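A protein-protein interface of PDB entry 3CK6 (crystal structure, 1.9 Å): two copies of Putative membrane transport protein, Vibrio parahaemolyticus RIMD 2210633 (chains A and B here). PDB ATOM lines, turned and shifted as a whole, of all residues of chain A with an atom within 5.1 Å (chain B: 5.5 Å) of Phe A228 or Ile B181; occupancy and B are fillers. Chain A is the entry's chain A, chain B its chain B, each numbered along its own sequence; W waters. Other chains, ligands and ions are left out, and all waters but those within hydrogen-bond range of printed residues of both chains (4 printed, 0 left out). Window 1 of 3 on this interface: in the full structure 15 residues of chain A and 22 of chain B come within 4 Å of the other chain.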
ATOM      1  N   GLU A 224      20.753 -15.727  22.966  1.00  0.00           N
ATOM      2  CA  GLU A 224      21.842 -15.001  22.281  1.00  0.00           C
ATOM      3  C   GLU A 224      21.548 -13.504  22.202  1.00  0.00           C
ATOM      4  O   GLU A 224      22.435 -12.654  22.396  1.00  0.00           O
ATOM      5  CB  GLU A 224      22.079 -15.618  20.891  1.00  0.00           C
ATOM      6  CG  GLU A 224      22.841 -16.928  20.970  1.00  0.00           C
ATOM      7  CD  GLU A 224      22.851 -17.721  19.673  1.00  0.00           C
ATOM      8  OE1 GLU A 224      22.196 -17.303  18.662  1.00  0.00           O
ATOM      9  OE2 GLU A 224      23.534 -18.776  19.674  1.00  0.00           O
ATOM     10  N   THR A 225      20.284 -13.181  21.960  1.00  0.00           N
ATOM     11  CA  THR A 225      19.864 -11.795  21.928  1.00  0.00           C
ATOM     12  C   THR A 225      20.024 -11.113  23.298  1.00  0.00           C
ATOM     13  O   THR A 225      20.458  -9.957  23.380  1.00  0.00           O
ATOM     14  CB  THR A 225      18.421 -11.664  21.413  1.00  0.00           C
ATOM     15  OG1 THR A 225      18.387 -12.044  20.029  1.00  0.00           O
ATOM     16  CG2 THR A 225      17.932 -10.189  21.536  1.00  0.00           C
ATOM     17  N   ILE A 226      19.644 -11.818  24.360  1.00  0.00           N
ATOM     18  CA  ILE A 226      19.819 -11.309  25.715  1.00  0.00           C
ATOM     19  C   ILE A 226      21.305 -11.002  26.006  1.00  0.00           C
ATOM     20  O   ILE A 226      21.619  -9.940  26.529  1.00  0.00           O
ATOM     21  CB  ILE A 226      19.191 -12.261  26.790  1.00  0.00           C
ATOM     22  CG1 ILE A 226      17.652 -12.181  26.707  1.00  0.00           C
ATOM     23  CG2 ILE A 226      19.713 -11.887  28.226  1.00  0.00           C
ATOM     24  CD1 ILE A 226      16.942 -13.321  27.429  1.00  0.00           C
ATOM     25  N   GLU A 227      22.204 -11.919  25.641  1.00  0.00           N
ATOM     26  CA  GLU A 227      23.648 -11.657  25.825  1.00  0.00           C
ATOM     27  C   GLU A 227      24.102 -10.437  25.051  1.00  0.00           C
ATOM     28  O   GLU A 227      24.906  -9.642  25.549  1.00  0.00           O
ATOM     29  CB  GLU A 227      24.487 -12.859  25.409  1.00  0.00           C
ATOM     30  CG  GLU A 227      24.317 -14.041  26.323  1.00  0.00           C
ATOM     31  CD  GLU A 227      24.805 -13.764  27.739  1.00  0.00           C
ATOM     32  OE1 GLU A 227      24.062 -14.118  28.669  1.00  0.00           O
ATOM     33  OE2 GLU A 227      25.909 -13.192  27.922  1.00  0.00           O
ATOM     34  N   PHE A 228      23.575 -10.267  23.833  1.00  0.00           N
ATOM     35  CA  PHE A 228      23.960  -9.102  23.022  1.00  0.00           C
ATOM     36  C   PHE A 228      23.516  -7.803  23.702  1.00  0.00           C
ATOM     37  O   PHE A 228      24.277  -6.833  23.758  1.00  0.00           O
ATOM     38  CB  PHE A 228      23.361  -9.198  21.614  1.00  0.00           C
ATOM     39  CG  PHE A 228      23.476  -7.935  20.820  1.00  0.00           C
ATOM     40  CD1 PHE A 228      24.719  -7.467  20.410  1.00  0.00           C
ATOM     41  CD2 PHE A 228      22.337  -7.214  20.468  1.00  0.00           C
ATOM     42  CE1 PHE A 228      24.823  -6.287  19.669  1.00  0.00           C
ATOM     43  CE2 PHE A 228      22.429  -6.036  19.726  1.00  0.00           C
ATOM     44  CZ  PHE A 228      23.673  -5.571  19.330  1.00  0.00           C
ATOM     45  N   TYR A 229      22.284  -7.799  24.210  1.00  0.00           N
ATOM     46  CA  TYR A 229      21.721  -6.618  24.876  1.00  0.00           C
ATOM     47  C   TYR A 229      22.492  -6.224  26.133  1.00  0.00           C
ATOM     48  O   TYR A 229      22.737  -5.043  26.364  1.00  0.00           O
ATOM     49  CB  TYR A 229      20.232  -6.833  25.187  1.00  0.00           C
ATOM     50  CG  TYR A 229      19.330  -6.816  23.970  1.00  0.00           C
ATOM     51  CD1 TYR A 229      19.783  -6.328  22.736  1.00  0.00           C
ATOM     52  CD2 TYR A 229      18.015  -7.259  24.053  1.00  0.00           C
ATOM     53  CE1 TYR A 229      18.959  -6.316  21.616  1.00  0.00           C
ATOM     54  CE2 TYR A 229      17.173  -7.233  22.943  1.00  0.00           C
ATOM     55  CZ  TYR A 229      17.655  -6.771  21.730  1.00  0.00           C
ATOM     56  OH  TYR A 229      16.822  -6.759  20.627  1.00  0.00           O
ATOM     57  N   LEU A 230      22.879  -7.219  26.925  1.00  0.00           N
ATOM     58  CA  LEU A 230      23.759  -7.014  28.078  1.00  0.00           C
ATOM     59  C   LEU A 230      25.113  -6.398  27.705  1.00  0.00           C
ATOM     60  O   LEU A 230      25.615  -5.511  28.407  1.00  0.00           O
ATOM     61  CB  LEU A 230      23.960  -8.336  28.829  1.00  0.00           C
ATOM     62  CG  LEU A 230      22.761  -8.792  29.666  1.00  0.00           C
ATOM     63  CD1 LEU A 230      22.971 -10.247  30.078  1.00  0.00           C
ATOM     64  CD2 LEU A 230      22.569  -7.841  30.886  1.00  0.00           C
ATOM     65  N   GLY A 231      25.689  -6.864  26.599  1.00  0.00           N
ATOM     66  CA  GLY A 231      26.883  -6.276  26.007  1.00  0.00           C
ATOM     67  C   GLY A 231      26.658  -4.836  25.565  1.00  0.00           C
ATOM     68  O   GLY A 231      27.547  -3.994  25.722  1.00  0.00           O
ATOM     69  N   GLU A 232      25.475  -4.541  25.029  1.00  0.00           N
ATOM     70  CA  GLU A 232      25.136  -3.159  24.669  1.00  0.00           C
ATOM     71  C   GLU A 232      25.022  -2.258  25.891  1.00  0.00           C
ATOM     72  O   GLU A 232      25.566  -1.145  25.896  1.00  0.00           O
ATOM     73  CB  GLU A 232      23.838  -3.092  23.868  1.00  0.00           C
ATOM     74  CG  GLU A 232      23.996  -3.402  22.387  1.00  0.00           C
ATOM     75  CD  GLU A 232      22.800  -2.904  21.581  1.00  0.00           C
ATOM     76  OE1 GLU A 232      22.976  -1.991  20.743  1.00  0.00           O
ATOM     77  OE2 GLU A 232      21.682  -3.407  21.811  1.00  0.00           O
ATOM     78  N   LEU A 235      28.552  -1.617  27.345  1.00  0.00           N
ATOM     79  CA  LEU A 235      29.197  -0.616  26.490  1.00  0.00           C
ATOM     80  C   LEU A 235      28.717   0.811  26.750  1.00  0.00           C
ATOM     81  O   LEU A 235      29.527   1.742  26.780  1.00  0.00           O
ATOM     82  CB  LEU A 235      28.921  -0.972  25.028  1.00  0.00           C
ATOM     83  CG  LEU A 235      29.351  -0.073  23.877  1.00  0.00           C
ATOM     84  CD1 LEU A 235      30.862  -0.007  23.775  1.00  0.00           C
ATOM     85  CD2 LEU A 235      28.771  -0.649  22.636  1.00  0.00           C
ATOM     86  N   ALA B 176      34.087   1.072  17.645  1.00  0.00           N
ATOM     87  CA  ALA B 176      34.696  -0.210  17.271  1.00  0.00           C
ATOM     88  C   ALA B 176      34.048  -1.371  18.032  1.00  0.00           C
ATOM     89  O   ALA B 176      33.617  -2.335  17.424  1.00  0.00           O
ATOM     90  CB  ALA B 176      36.203  -0.174  17.522  1.00  0.00           C
ATOM     91  N   GLN B 177      33.983  -1.249  19.360  1.00  0.00           N
ATOM     92  CA  GLN B 177      33.354  -2.236  20.234  1.00  0.00           C
ATOM     93  C   GLN B 177      31.900  -2.531  19.876  1.00  0.00           C
ATOM     94  O   GLN B 177      31.510  -3.710  19.831  1.00  0.00           O
ATOM     95  CB  GLN B 177      33.430  -1.798  21.692  1.00  0.00           C
ATOM     96  CG  GLN B 177      33.057  -2.910  22.677  1.00  0.00           C
ATOM     97  CD  GLN B 177      33.304  -2.521  24.134  1.00  0.00           C
ATOM     98  OE1 GLN B 177      32.894  -3.243  25.055  1.00  0.00           O
ATOM     99  NE2 GLN B 177      33.976  -1.388  24.352  1.00  0.00           N
ATOM    100  N   LYS B 178      31.118  -1.471  19.645  1.00  0.00           N
ATOM    101  CA  LYS B 178      29.713  -1.590  19.187  1.00  0.00           C
ATOM    102  C   LYS B 178      29.596  -2.483  17.954  1.00  0.00           C
ATOM    103  O   LYS B 178      28.739  -3.366  17.892  1.00  0.00           O
ATOM    104  CB  LYS B 178      29.092  -0.208  18.863  1.00  0.00           C
ATOM    105  CG  LYS B 178      28.867   0.732  20.054  1.00  0.00           C
ATOM    106  CD  LYS B 178      27.677   1.706  19.831  1.00  0.00           C
ATOM    107  CE  LYS B 178      27.347   2.553  21.081  1.00  0.00           C
ATOM    108  NZ  LYS B 178      28.046   3.884  21.163  1.00  0.00           N
ATOM    109  N   ALA B 179      30.446  -2.208  16.966  1.00  0.00           N
ATOM    110  CA  ALA B 179      30.459  -2.916  15.695  1.00  0.00           C
ATOM    111  C   ALA B 179      30.842  -4.389  15.875  1.00  0.00           C
ATOM    112  O   ALA B 179      30.166  -5.276  15.350  1.00  0.00           O
ATOM    113  CB  ALA B 179      31.424  -2.222  14.748  1.00  0.00           C
ATOM    114  N   LEU B 180      31.904  -4.622  16.651  1.00  0.00           N
ATOM    115  CA  LEU B 180      32.434  -5.941  16.942  1.00  0.00           C
ATOM    116  C   LEU B 180      31.429  -6.828  17.643  1.00  0.00           C
ATOM    117  O   LEU B 180      31.235  -7.967  17.218  1.00  0.00           O
ATOM    118  CB  LEU B 180      33.716  -5.866  17.771  1.00  0.00           C
ATOM    119  CG  LEU B 180      34.984  -5.438  17.018  1.00  0.00           C
ATOM    120  CD1 LEU B 180      36.074  -5.044  17.996  1.00  0.00           C
ATOM    121  CD2 LEU B 180      35.478  -6.525  16.070  1.00  0.00           C
ATOM    122  N   ILE B 181      30.774  -6.303  18.682  1.00  0.00           N
ATOM    123  CA  ILE B 181      29.774  -7.097  19.401  1.00  0.00           C
ATOM    124  C   ILE B 181      28.515  -7.345  18.548  1.00  0.00           C
ATOM    125  O   ILE B 181      27.905  -8.411  18.656  1.00  0.00           O
ATOM    126  CB  ILE B 181      29.407  -6.574  20.838  1.00  0.00           C
ATOM    127  CG1 ILE B 181      28.519  -5.331  20.787  1.00  0.00           C
ATOM    128  CG2 ILE B 181      30.672  -6.398  21.732  1.00  0.00           C
ATOM    129  CD1 ILE B 181      27.828  -5.051  22.097  1.00  0.00           C
ATOM    130  N   SER B 182      28.155  -6.390  17.688  1.00  0.00           N
ATOM    131  CA  SER B 182      27.045  -6.615  16.746  1.00  0.00           C
ATOM    132  C   SER B 182      27.357  -7.739  15.750  1.00  0.00           C
ATOM    133  O   SER B 182      26.485  -8.562  15.480  1.00  0.00           O
ATOM    134  CB  SER B 182      26.635  -5.335  16.009  1.00  0.00           C
ATOM    135  OG  SER B 182      26.278  -4.299  16.922  1.00  0.00           O
ATOM    136  N   ILE B 183      28.572  -7.768  15.197  1.00  0.00           N
ATOM    137  CA  ILE B 183      29.042  -8.881  14.336  1.00  0.00           C
ATOM    138  C   ILE B 183      29.094 -10.239  15.079  1.00  0.00           C
ATOM    139  O   ILE B 183      28.636 -11.272  14.562  1.00  0.00           O
ATOM    140  CB  ILE B 183      30.479  -8.620  13.719  1.00  0.00           C
ATOM    141  CG1 ILE B 183      30.556  -7.325  12.932  1.00  0.00           C
ATOM    142  CG2 ILE B 183      30.912  -9.789  12.796  1.00  0.00           C
ATOM    143  CD1 ILE B 183      29.509  -7.163  11.861  1.00  0.00           C
ATOM    144  N   LYS B 184      29.706 -10.229  16.269  1.00  0.00           N
ATOM    145  CA  LYS B 184      29.877 -11.427  17.089  1.00  0.00           C
ATOM    146  C   LYS B 184      28.553 -12.136  17.373  1.00  0.00           C
ATOM    147  O   LYS B 184      28.471 -13.368  17.307  1.00  0.00           O
ATOM    148  CB  LYS B 184      30.566 -11.071  18.405  1.00  0.00           C
ATOM    149  CG  LYS B 184      30.869 -12.260  19.315  1.00  0.00           C
ATOM    150  CD  LYS B 184      31.668 -11.818  20.557  1.00  0.00           C
ATOM    151  CE  LYS B 184      31.761 -12.949  21.579  1.00  0.00           C
ATOM    152  NZ  LYS B 184      32.427 -12.460  22.838  1.00  0.00           N
ATOM    153  N   ARG B 185      27.538 -11.354  17.721  1.00  0.00           N
ATOM    154  CA  ARG B 185      26.163 -11.848  17.871  1.00  0.00           C
ATOM    155  C   ARG B 185      25.762 -12.947  16.863  1.00  0.00           C
ATOM    156  O   ARG B 185      25.112 -13.929  17.233  1.00  0.00           O
ATOM    157  CB  ARG B 185      25.191 -10.677  17.752  1.00  0.00           C
ATOM    158  CG  ARG B 185      23.762 -11.005  18.139  1.00  0.00           C
ATOM    159  CD  ARG B 185      22.865  -9.839  17.820  1.00  0.00           C
ATOM    160  NE  ARG B 185      21.472 -10.141  18.141  1.00  0.00           N
ATOM    161  CZ  ARG B 185      20.475  -9.303  17.941  1.00  0.00           C
ATOM    162  NH1 ARG B 185      20.728  -8.102  17.443  1.00  0.00           N
ATOM    163  NH2 ARG B 185      19.237  -9.651  18.274  1.00  0.00           N
ATOM    164  N   LEU B 230      38.448  -7.266  20.170  1.00  0.00           N
ATOM    165  CA  LEU B 230      37.710  -6.897  21.391  1.00  0.00           C
ATOM    166  C   LEU B 230      38.684  -6.746  22.576  1.00  0.00           C
ATOM    167  O   LEU B 230      38.562  -5.821  23.404  1.00  0.00           O
ATOM    168  CB  LEU B 230      36.601  -7.943  21.656  1.00  0.00           C
ATOM    169  CG  LEU B 230      35.261  -7.785  20.892  1.00  0.00           C
ATOM    170  CD1 LEU B 230      34.405  -9.024  21.074  1.00  0.00           C
ATOM    171  CD2 LEU B 230      34.473  -6.540  21.332  1.00  0.00           C
HETATM  172  O   HOH W   1      22.272 -14.741  17.345  1.00  0.00           O
HETATM  173  O   HOH W   2      30.025  -4.566  25.701  1.00  0.00           O
HETATM  174  O   HOH W   3      17.397  -7.974  17.884  1.00  0.00           O
HETATM  175  O   HOH W   4      20.466 -13.037  18.367  1.00  0.00           O
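The side-chain hydroxyl (OG1) of Thr A225 is in hydrogen-bond range of the guanidinium group (NH2) of Arg B185, at 3.1 Å.
O of Lys B178 lies within hydrogen-bond range of OG of Ser B182.
Among the printed residues, merely in contact across the chains: Phe A228 with Ile B181 (3.8 Å), Phe A228 with Ser B182 (3.7 Å), Phe A228 with Arg B185 (3.5 Å), Gly A231 with Ile B181 (3.7 Å), Glu A232 with Ile B181 (3.8 Å), Leu A235 with Gln B177 (3.5 Å) and Leu A235 with Lys B178 (2.9 Å).
Phe A228 touches just these residues of chain B: Ile B181, Ser B182 and Arg B185. Ile B181 touches just these residues of chain A: Phe A228 (3.8 Å), Gly A231 (3.7 Å) and Glu A232 (3.8 Å). Of the printed residues of chain A, Ser B182 touches Phe A228 (3.7 Å). Printed residues of chain A within 4 Å of Lys B178: Leu A235 (2.9 Å). Ile A226 touches none of the printed residues of chain B. The nearest residue of chain B that does not touch Phe A228 is Lys B178 (5.2 Å).
Hydrophobic or aromatic side chains of chain A within 4 Å of the printed part of chain B: Phe A228 and Leu A235. Among the printed residues, 8 pairs touch across the chains. Among the printed residues, no Asp or Glu carboxylate lies within 4 Å of a Lys or Arg side-chain nitrogen of the other chain.
Position printed for both chains: 230. Of the 8 pairs that touch across the chains among the printed residues, none has its exchanged pair printed and touching as well.
Water W3 bridges NH2 of Arg B185 (2.5 Å) and OH of Tyr A229 (3.1 Å). Water W2 lies within hydrogen-bond range of the backbone carbonyl oxygen (O) of Gly A231 and the side-chain amide oxygen (OE1) of Gln B177. Water W4 lies within hydrogen-bond range of the side-chain hydroxyl (OG1) of Thr A225 and the guanidinium group (NE) of Arg B185. Water W1 bridges the side-chain carboxylate (OE1) of Glu A224 (2.9 Å) and the backbone carbonyl oxygen (O) of Arg B185 (3.0 Å).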
